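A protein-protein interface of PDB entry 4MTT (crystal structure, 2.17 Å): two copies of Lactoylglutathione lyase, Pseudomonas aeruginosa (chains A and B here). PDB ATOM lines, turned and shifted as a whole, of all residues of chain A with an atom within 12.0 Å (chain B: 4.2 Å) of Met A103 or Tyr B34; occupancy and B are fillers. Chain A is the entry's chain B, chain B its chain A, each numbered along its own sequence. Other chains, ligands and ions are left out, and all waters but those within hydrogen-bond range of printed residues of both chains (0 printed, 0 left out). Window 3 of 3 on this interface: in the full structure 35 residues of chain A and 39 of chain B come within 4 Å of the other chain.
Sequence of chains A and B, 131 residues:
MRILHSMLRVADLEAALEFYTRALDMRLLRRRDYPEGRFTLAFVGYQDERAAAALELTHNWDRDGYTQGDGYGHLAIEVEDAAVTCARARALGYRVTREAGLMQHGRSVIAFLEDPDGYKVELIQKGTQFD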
ATOM      1  N   HIS A  74      -5.138  17.850  13.019  1.00  0.00           N
ATOM      2  CA  HIS A  74      -5.061  16.393  12.922  1.00  0.00           C
ATOM      3  C   HIS A  74      -4.187  15.981  11.729  1.00  0.00           C
ATOM      4  O   HIS A  74      -3.759  16.822  10.936  1.00  0.00           O
ATOM      5  CB  HIS A  74      -6.497  15.806  12.750  1.00  0.00           C
ATOM      6  CG  HIS A  74      -7.259  16.371  11.572  1.00  0.00           C
ATOM      7  ND1 HIS A  74      -8.345  17.236  11.747  1.00  0.00           N
ATOM      8  CD2 HIS A  74      -7.104  16.132  10.245  1.00  0.00           C
ATOM      9  CE1 HIS A  74      -8.807  17.487  10.533  1.00  0.00           C
ATOM     10  NE2 HIS A  74      -8.076  16.865   9.591  1.00  0.00           N
ATOM     11  N   ARG A  98     -16.563   9.755  16.509  1.00  0.00           N
ATOM     12  CA  ARG A  98     -17.140   9.850  15.167  1.00  0.00           C
ATOM     13  C   ARG A  98     -17.963  11.126  15.047  1.00  0.00           C
ATOM     14  O   ARG A  98     -18.678  11.510  15.992  1.00  0.00           O
ATOM     15  CB  ARG A  98     -17.982   8.612  14.813  1.00  0.00           C
ATOM     16  CG  ARG A  98     -17.200   7.316  14.931  1.00  0.00           C
ATOM     17  CD  ARG A  98     -18.092   6.134  14.826  1.00  0.00           C
ATOM     18  NE  ARG A  98     -18.336   5.808  13.430  1.00  0.00           N
ATOM     19  CZ  ARG A  98     -19.353   5.076  13.005  1.00  0.00           C
ATOM     20  NH1 ARG A  98     -20.224   4.570  13.872  1.00  0.00           N
ATOM     21  NH2 ARG A  98     -19.521   4.858  11.707  1.00  0.00           N
ATOM     22  N   GLU A  99     -17.838  11.791  13.885  1.00  0.00           N
ATOM     23  CA  GLU A  99     -18.548  13.037  13.616  1.00  0.00           C
ATOM     24  C   GLU A  99     -19.448  12.877  12.407  1.00  0.00           C
ATOM     25  O   GLU A  99     -18.993  12.438  11.341  1.00  0.00           O
ATOM     26  CB  GLU A  99     -17.569  14.195  13.337  1.00  0.00           C
ATOM     27  CG  GLU A  99     -16.365  14.280  14.259  1.00  0.00           C
ATOM     28  CD  GLU A  99     -16.564  15.100  15.510  1.00  0.00           C
ATOM     29  OE1 GLU A  99     -17.656  15.686  15.673  1.00  0.00           O
ATOM     30  OE2 GLU A  99     -15.612  15.174  16.319  1.00  0.00           O
ATOM     31  N   ALA A 100     -20.714  13.278  12.559  1.00  0.00           N
ATOM     32  CA  ALA A 100     -21.660  13.259  11.453  1.00  0.00           C
ATOM     33  C   ALA A 100     -22.029  14.713  11.090  1.00  0.00           C
ATOM     34  O   ALA A 100     -22.122  15.562  11.972  1.00  0.00           O
ATOM     35  CB  ALA A 100     -22.897  12.468  11.835  1.00  0.00           C
ATOM     36  N   GLY A 101     -22.240  14.973   9.806  1.00  0.00           N
ATOM     37  CA  GLY A 101     -22.636  16.294   9.321  1.00  0.00           C
ATOM     38  C   GLY A 101     -21.508  17.276   9.058  1.00  0.00           C
ATOM     39  O   GLY A 101     -21.766  18.478   8.954  1.00  0.00           O
ATOM     40  N   LEU A 102     -20.248  16.789   8.956  1.00  0.00           N
ATOM     41  CA  LEU A 102     -19.108  17.665   8.643  1.00  0.00           C
ATOM     42  C   LEU A 102     -19.323  18.015   7.180  1.00  0.00           C
ATOM     43  O   LEU A 102     -19.240  17.129   6.323  1.00  0.00           O
ATOM     44  CB  LEU A 102     -17.722  16.985   8.881  1.00  0.00           C
ATOM     45  CG  LEU A 102     -17.337  16.674  10.346  1.00  0.00           C
ATOM     46  CD1 LEU A 102     -16.041  15.801  10.435  1.00  0.00           C
ATOM     47  CD2 LEU A 102     -17.234  17.959  11.223  1.00  0.00           C
ATOM     48  N   MET A 103     -19.775  19.258   6.920  1.00  0.00           N
ATOM     49  CA  MET A 103     -20.095  19.725   5.561  1.00  0.00           C
ATOM     50  C   MET A 103     -18.969  19.574   4.549  1.00  0.00           C
ATOM     51  O   MET A 103     -19.238  19.468   3.361  1.00  0.00           O
ATOM     52  CB  MET A 103     -20.832  21.083   5.501  1.00  0.00           C
ATOM     53  CG  MET A 103     -20.289  22.123   6.425  1.00  0.00           C
ATOM     54  SD  MET A 103     -21.397  23.531   6.633  1.00  0.00           S
ATOM     55  CE  MET A 103     -22.676  22.844   7.723  1.00  0.00           C
ATOM     56  N   GLN A 104     -17.727  19.451   5.037  1.00  0.00           N
ATOM     57  CA  GLN A 104     -16.553  19.198   4.208  1.00  0.00           C
ATOM     58  C   GLN A 104     -16.451  17.719   3.822  1.00  0.00           C
ATOM     59  O   GLN A 104     -15.667  17.378   2.942  1.00  0.00           O
ATOM     60  CB  GLN A 104     -15.260  19.719   4.858  1.00  0.00           C
ATOM     61  CG  GLN A 104     -14.821  19.054   6.181  1.00  0.00           C
ATOM     62  CD  GLN A 104     -15.468  19.675   7.396  1.00  0.00           C
ATOM     63  OE1 GLN A 104     -16.688  19.851   7.474  1.00  0.00           O
ATOM     64  NE2 GLN A 104     -14.668  20.009   8.388  1.00  0.00           N
ATOM     65  N   HIS A 105     -17.263  16.847   4.441  1.00  0.00           N
ATOM     66  CA  HIS A 105     -17.228  15.409   4.117  1.00  0.00           C
ATOM     67  C   HIS A 105     -18.570  14.852   3.553  1.00  0.00           C
ATOM     68  O   HIS A 105     -18.788  13.634   3.569  1.00  0.00           O
ATOM     69  CB  HIS A 105     -16.684  14.586   5.302  1.00  0.00           C
ATOM     70  CG  HIS A 105     -15.269  14.929   5.682  1.00  0.00           C
ATOM     71  ND1 HIS A 105     -14.177  14.441   4.956  1.00  0.00           N
ATOM     72  CD2 HIS A 105     -14.803  15.664   6.724  1.00  0.00           C
ATOM     73  CE1 HIS A 105     -13.099  14.920   5.564  1.00  0.00           C
ATOM     74  NE2 HIS A 105     -13.420  15.654   6.633  1.00  0.00           N
ATOM     75  N   GLY A 106     -19.425  15.746   3.034  1.00  0.00           N
ATOM     76  CA  GLY A 106     -20.720  15.399   2.449  1.00  0.00           C
ATOM     77  C   GLY A 106     -21.667  14.666   3.384  1.00  0.00           C
ATOM     78  O   GLY A 106     -22.119  15.227   4.386  1.00  0.00           O
ATOM     79  N   ARG A 107     -21.965  13.399   3.066  1.00  0.00           N
ATOM     80  CA  ARG A 107     -22.848  12.539   3.870  1.00  0.00           C
ATOM     81  C   ARG A 107     -22.045  11.519   4.698  1.00  0.00           C
ATOM     82  O   ARG A 107     -22.650  10.715   5.418  1.00  0.00           O
ATOM     83  CB  ARG A 107     -23.860  11.802   2.965  1.00  0.00           C
ATOM     84  CG  ARG A 107     -25.026  12.670   2.511  1.00  0.00           C
ATOM     85  CD  ARG A 107     -25.652  12.126   1.238  1.00  0.00           C
ATOM     86  NE  ARG A 107     -26.907  12.807   0.916  1.00  0.00           N
ATOM     87  CZ  ARG A 107     -28.106  12.406   1.328  1.00  0.00           C
ATOM     88  NH1 ARG A 107     -28.229  11.317   2.079  1.00  0.00           N
ATOM     89  NH2 ARG A 107     -29.193  13.089   0.991  1.00  0.00           N
ATOM     90  N   SER A 108     -20.690  11.549   4.604  1.00  0.00           N
ATOM     91  CA  SER A 108     -19.855  10.606   5.335  1.00  0.00           C
ATOM     92  C   SER A 108     -19.756  10.938   6.826  1.00  0.00           C
ATOM     93  O   SER A 108     -19.593  12.105   7.213  1.00  0.00           O
ATOM     94  CB  SER A 108     -18.448  10.528   4.750  1.00  0.00           C
ATOM     95  OG  SER A 108     -18.428  10.206   3.371  1.00  0.00           O
ATOM     96  N   VAL A 109     -19.791   9.884   7.651  1.00  0.00           N
ATOM     97  CA  VAL A 109     -19.565   9.988   9.084  1.00  0.00           C
ATOM     98  C   VAL A 109     -18.067   9.745   9.181  1.00  0.00           C
ATOM     99  O   VAL A 109     -17.573   8.758   8.637  1.00  0.00           O
ATOM    100  CB  VAL A 109     -20.409   8.952   9.880  1.00  0.00           C
ATOM    101  CG1 VAL A 109     -19.863   8.743  11.286  1.00  0.00           C
ATOM    102  CG2 VAL A 109     -21.883   9.359   9.911  1.00  0.00           C
ATOM    103  N   ILE A 110     -17.340  10.660   9.789  1.00  0.00           N
ATOM    104  CA  ILE A 110     -15.871  10.527   9.878  1.00  0.00           C
ATOM    105  C   ILE A 110     -15.422  10.126  11.256  1.00  0.00           C
ATOM    106  O   ILE A 110     -15.792  10.769  12.241  1.00  0.00           O
ATOM    107  CB  ILE A 110     -15.152  11.829   9.381  1.00  0.00           C
ATOM    108  CG1 ILE A 110     -15.606  12.224   7.946  1.00  0.00           C
ATOM    109  CG2 ILE A 110     -13.601  11.791   9.544  1.00  0.00           C
ATOM    110  CD1 ILE A 110     -15.186  11.287   6.769  1.00  0.00           C
ATOM    111  N   PHE A 112     -12.344   9.583  14.073  1.00  0.00           N
ATOM    112  CA  PHE A 112     -11.103  10.181  14.531  1.00  0.00           C
ATOM    113  C   PHE A 112     -10.485   9.289  15.619  1.00  0.00           C
ATOM    114  O   PHE A 112     -11.141   8.961  16.620  1.00  0.00           O
ATOM    115  CB  PHE A 112     -11.319  11.609  15.063  1.00  0.00           C
ATOM    116  CG  PHE A 112     -11.657  12.630  13.994  1.00  0.00           C
ATOM    117  CD1 PHE A 112     -10.664  13.435  13.434  1.00  0.00           C
ATOM    118  CD2 PHE A 112     -12.970  12.805  13.563  1.00  0.00           C
ATOM    119  CE1 PHE A 112     -10.982  14.389  12.453  1.00  0.00           C
ATOM    120  CE2 PHE A 112     -13.283  13.752  12.581  1.00  0.00           C
ATOM    121  CZ  PHE A 112     -12.288  14.530  12.029  1.00  0.00           C
ATOM    122  N   GLU A 122      -7.445  11.522  11.630  1.00  0.00           N
ATOM    123  CA  GLU A 122      -8.635  11.470  10.803  1.00  0.00           C
ATOM    124  C   GLU A 122      -8.616  10.286   9.852  1.00  0.00           C
ATOM    125  O   GLU A 122      -7.666  10.106   9.084  1.00  0.00           O
ATOM    126  CB  GLU A 122      -8.806  12.803  10.069  1.00  0.00           C
ATOM    127  CG  GLU A 122      -9.920  12.810   9.044  1.00  0.00           C
ATOM    128  CD  GLU A 122     -10.165  14.194   8.493  1.00  0.00           C
ATOM    129  OE1 GLU A 122      -9.243  14.769   7.871  1.00  0.00           O
ATOM    130  OE2 GLU A 122     -11.265  14.729   8.745  1.00  0.00           O
ATOM    131  N   ILE A 124     -10.034   8.498   6.635  1.00  0.00           N
ATOM    132  CA  ILE A 124     -10.736   8.720   5.386  1.00  0.00           C
ATOM    133  C   ILE A 124     -10.722   7.395   4.618  1.00  0.00           C
ATOM    134  O   ILE A 124      -9.661   6.836   4.313  1.00  0.00           O
ATOM    135  CB  ILE A 124     -10.202   9.940   4.594  1.00  0.00           C
ATOM    136  CG1 ILE A 124     -10.509  11.259   5.377  1.00  0.00           C
ATOM    137  CG2 ILE A 124     -10.822   9.986   3.163  1.00  0.00           C
ATOM    138  CD1 ILE A 124      -9.629  12.418   5.128  1.00  0.00           C
ATOM    139  N   ARG B  32     -12.724  25.316  -0.049  1.00  0.00           N
ATOM    140  CA  ARG B  32     -14.165  25.224   0.169  1.00  0.00           C
ATOM    141  C   ARG B  32     -14.542  26.169   1.324  1.00  0.00           C
ATOM    142  O   ARG B  32     -13.956  26.084   2.400  1.00  0.00           O
ATOM    143  CB  ARG B  32     -14.672  23.783   0.457  1.00  0.00           C
ATOM    144  CG  ARG B  32     -14.335  22.653  -0.552  1.00  0.00           C
ATOM    145  CD  ARG B  32     -15.168  22.668  -1.826  1.00  0.00           C
ATOM    146  NE  ARG B  32     -14.753  21.606  -2.753  1.00  0.00           N
ATOM    147  CZ  ARG B  32     -13.892  21.749  -3.758  1.00  0.00           C
ATOM    148  NH1 ARG B  32     -13.325  22.928  -3.999  1.00  0.00           N
ATOM    149  NH2 ARG B  32     -13.597  20.722  -4.535  1.00  0.00           N
ATOM    150  N   ASP B  33     -15.502  27.088   1.065  1.00  0.00           N
ATOM    151  CA  ASP B  33     -16.006  28.061   2.017  1.00  0.00           C
ATOM    152  C   ASP B  33     -17.435  27.693   2.293  1.00  0.00           C
ATOM    153  O   ASP B  33     -18.213  27.579   1.351  1.00  0.00           O
ATOM    154  CB  ASP B  33     -15.964  29.485   1.435  1.00  0.00           C
ATOM    155  CG  ASP B  33     -14.586  30.075   1.344  1.00  0.00           C
ATOM    156  OD1 ASP B  33     -13.817  29.648   0.461  1.00  0.00           O
ATOM    157  OD2 ASP B  33     -14.305  31.037   2.087  1.00  0.00           O
ATOM    158  N   TYR B  34     -17.782  27.506   3.563  1.00  0.00           N
ATOM    159  CA  TYR B  34     -19.130  27.080   3.918  1.00  0.00           C
ATOM    160  C   TYR B  34     -19.839  28.151   4.728  1.00  0.00           C
ATOM    161  O   TYR B  34     -19.595  28.238   5.934  1.00  0.00           O
ATOM    162  CB  TYR B  34     -19.110  25.742   4.694  1.00  0.00           C
ATOM    163  CG  TYR B  34     -18.441  24.615   3.944  1.00  0.00           C
ATOM    164  CD1 TYR B  34     -19.153  23.838   3.030  1.00  0.00           C
ATOM    165  CD2 TYR B  34     -17.097  24.318   4.146  1.00  0.00           C
ATOM    166  CE1 TYR B  34     -18.534  22.809   2.325  1.00  0.00           C
ATOM    167  CE2 TYR B  34     -16.477  23.271   3.466  1.00  0.00           C
ATOM    168  CZ  TYR B  34     -17.204  22.508   2.572  1.00  0.00           C
ATOM    169  OH  TYR B  34     -16.583  21.487   1.895  1.00  0.00           O
ATOM    170  N   PRO B  35     -20.697  28.993   4.086  1.00  0.00           N
ATOM    171  CA  PRO B  35     -21.441  30.007   4.865  1.00  0.00           C
ATOM    172  C   PRO B  35     -22.324  29.362   5.957  1.00  0.00           C
ATOM    173  O   PRO B  35     -22.508  29.950   7.018  1.00  0.00           O
ATOM    174  CB  PRO B  35     -22.263  30.755   3.791  1.00  0.00           C
ATOM    175  CG  PRO B  35     -22.342  29.825   2.618  1.00  0.00           C
ATOM    176  CD  PRO B  35     -21.067  29.018   2.650  1.00  0.00           C
ATOM    177  N   GLU B  36     -22.804  28.130   5.722  1.00  0.00           N
ATOM    178  CA  GLU B  36     -23.664  27.364   6.636  1.00  0.00           C
ATOM    179  C   GLU B  36     -22.925  26.988   7.911  1.00  0.00           C
ATOM    180  O   GLU B  36     -23.519  27.021   8.975  1.00  0.00           O
ATOM    181  CB  GLU B  36     -24.241  26.099   5.965  1.00  0.00           C
ATOM    182  CG  GLU B  36     -24.873  26.315   4.599  1.00  0.00           C
ATOM    183  CD  GLU B  36     -23.955  26.210   3.387  1.00  0.00           C
ATOM    184  OE1 GLU B  36     -22.711  26.168   3.558  1.00  0.00           O
ATOM    185  OE2 GLU B  36     -24.489  26.173   2.254  1.00  0.00           O
ATOM    186  N   GLY B  37     -21.634  26.677   7.807  1.00  0.00           N
ATOM    187  CA  GLY B  37     -20.819  26.332   8.966  1.00  0.00           C
ATOM    188  C   GLY B  37     -19.874  27.428   9.418  1.00  0.00           C
ATOM    189  O   GLY B  37     -19.217  27.283  10.451  1.00  0.00           O
ATOM    190  N   ARG B  38     -19.789  28.531   8.645  1.00  0.00           N
ATOM    191  CA  ARG B  38     -18.902  29.690   8.895  1.00  0.00           C
ATOM    192  C   ARG B  38     -17.443  29.344   9.052  1.00  0.00           C
ATOM    193  O   ARG B  38     -16.760  29.810   9.961  1.00  0.00           O
ATOM    194  CB  ARG B  38     -19.413  30.587  10.020  1.00  0.00           C
ATOM    195  CG  ARG B  38     -20.772  31.158   9.667  1.00  0.00           C
ATOM    196  CD  ARG B  38     -21.201  32.219  10.620  1.00  0.00           C
ATOM    197  NE  ARG B  38     -20.308  33.371  10.637  1.00  0.00           N
ATOM    198  CZ  ARG B  38     -20.375  34.382   9.783  1.00  0.00           C
ATOM    199  NH1 ARG B  38     -21.272  34.379   8.816  1.00  0.00           N
ATOM    200  NH2 ARG B  38     -19.537  35.407   9.892  1.00  0.00           N
ATOM    201  N   PHE B  39     -16.966  28.529   8.143  1.00  0.00           N
ATOM    202  CA  PHE B  39     -15.571  28.133   8.116  1.00  0.00           C
ATOM    203  C   PHE B  39     -15.150  27.895   6.693  1.00  0.00           C
ATOM    204  O   PHE B  39     -15.991  27.643   5.841  1.00  0.00           O
ATOM    205  CB  PHE B  39     -15.296  26.899   9.001  1.00  0.00           C
ATOM    206  CG  PHE B  39     -15.703  25.577   8.407  1.00  0.00           C
ATOM    207  CD1 PHE B  39     -14.769  24.772   7.757  1.00  0.00           C
ATOM    208  CD2 PHE B  39     -17.009  25.118   8.527  1.00  0.00           C
ATOM    209  CE1 PHE B  39     -15.135  23.532   7.237  1.00  0.00           C
ATOM    210  CE2 PHE B  39     -17.388  23.887   7.977  1.00  0.00           C
ATOM    211  CZ  PHE B  39     -16.443  23.092   7.355  1.00  0.00           C
ATOM    212  N   TRP B  61     -14.398  31.544  10.578  1.00  0.00           N
ATOM    213  CA  TRP B  61     -14.729  32.945  10.321  1.00  0.00           C
ATOM    214  C   TRP B  61     -14.908  33.787  11.581  1.00  0.00           C
ATOM    215  O   TRP B  61     -14.585  34.970  11.558  1.00  0.00           O
ATOM    216  CB  TRP B  61     -15.989  33.061   9.445  1.00  0.00           C
ATOM    217  CG  TRP B  61     -15.951  32.383   8.094  1.00  0.00           C
ATOM    218  CD1 TRP B  61     -14.956  31.600   7.583  1.00  0.00           C
ATOM    219  CD2 TRP B  61     -17.029  32.328   7.149  1.00  0.00           C
ATOM    220  NE1 TRP B  61     -15.321  31.116   6.350  1.00  0.00           N
ATOM    221  CE2 TRP B  61     -16.581  31.572   6.046  1.00  0.00           C
ATOM    222  CE3 TRP B  61     -18.310  32.913   7.098  1.00  0.00           C
ATOM    223  CZ2 TRP B  61     -17.356  31.398   4.889  1.00  0.00           C
ATOM    224  CZ3 TRP B  61     -19.083  32.733   5.960  1.00  0.00           C
ATOM    225  CH2 TRP B  61     -18.603  31.986   4.870  1.00  0.00           C
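Of the 17 printed residues of chain A, 2 touch a printed residue of chain B. Printed residues of chain A that touch a printed residue of chain B: Met A103 and Gln A104. Of the 9 printed residues of chain B, 4 touch a printed residue of chain A. Among the printed residues, 6 pairs touch across the chains. Among the printed residues, no Asp or Glu carboxylate lies within 4 Å of a Lys or Arg side-chain nitrogen of the other chain.
Leu A102 touches none of the printed residues of chain B. Met A103 touches four residues of chain B. Of the printed residues of chain B, Gln A104 touches Tyr B34 and Phe B39. Glu A122 touches none of the printed residues of chain B. No residue of chain A comes within 4 Å of Arg B32. No residue of chain A comes within 4 Å of Asp B33. Printed residues of chain A within 4 Å of Tyr B34: Met A103 and Gln A104. Glu B36 touches just one residue of chain A: Met A103. Printed residues of chain A within 4 Å of Gly B37: Met A103. Of the printed residues of chain A, Phe B39 touches Met A103 (3.7 Å) and Gln A104 (3.3 Å). The nearest printed residue of chain B that does not touch Gln A104 is Arg B32 (6.0 Å).
Among the printed residues, merely in contact across the chains: Met A103 with Tyr B34, Met A103 with Glu B36, Met A103 with Phe B39, Gln A104 with Tyr B34 and Gln A104 with Phe B39.
The side-chain sulfur of Met A103 lies within hydrogen-bond range of the backbone NH of Gly B37 (3.4 Å).
The backbone NH (N) of Tyr B34 lies within hydrogen-bond range of the backbone carbonyl oxygen (O) of Phe B39 (2.9 Å).
No position is printed for both chains.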
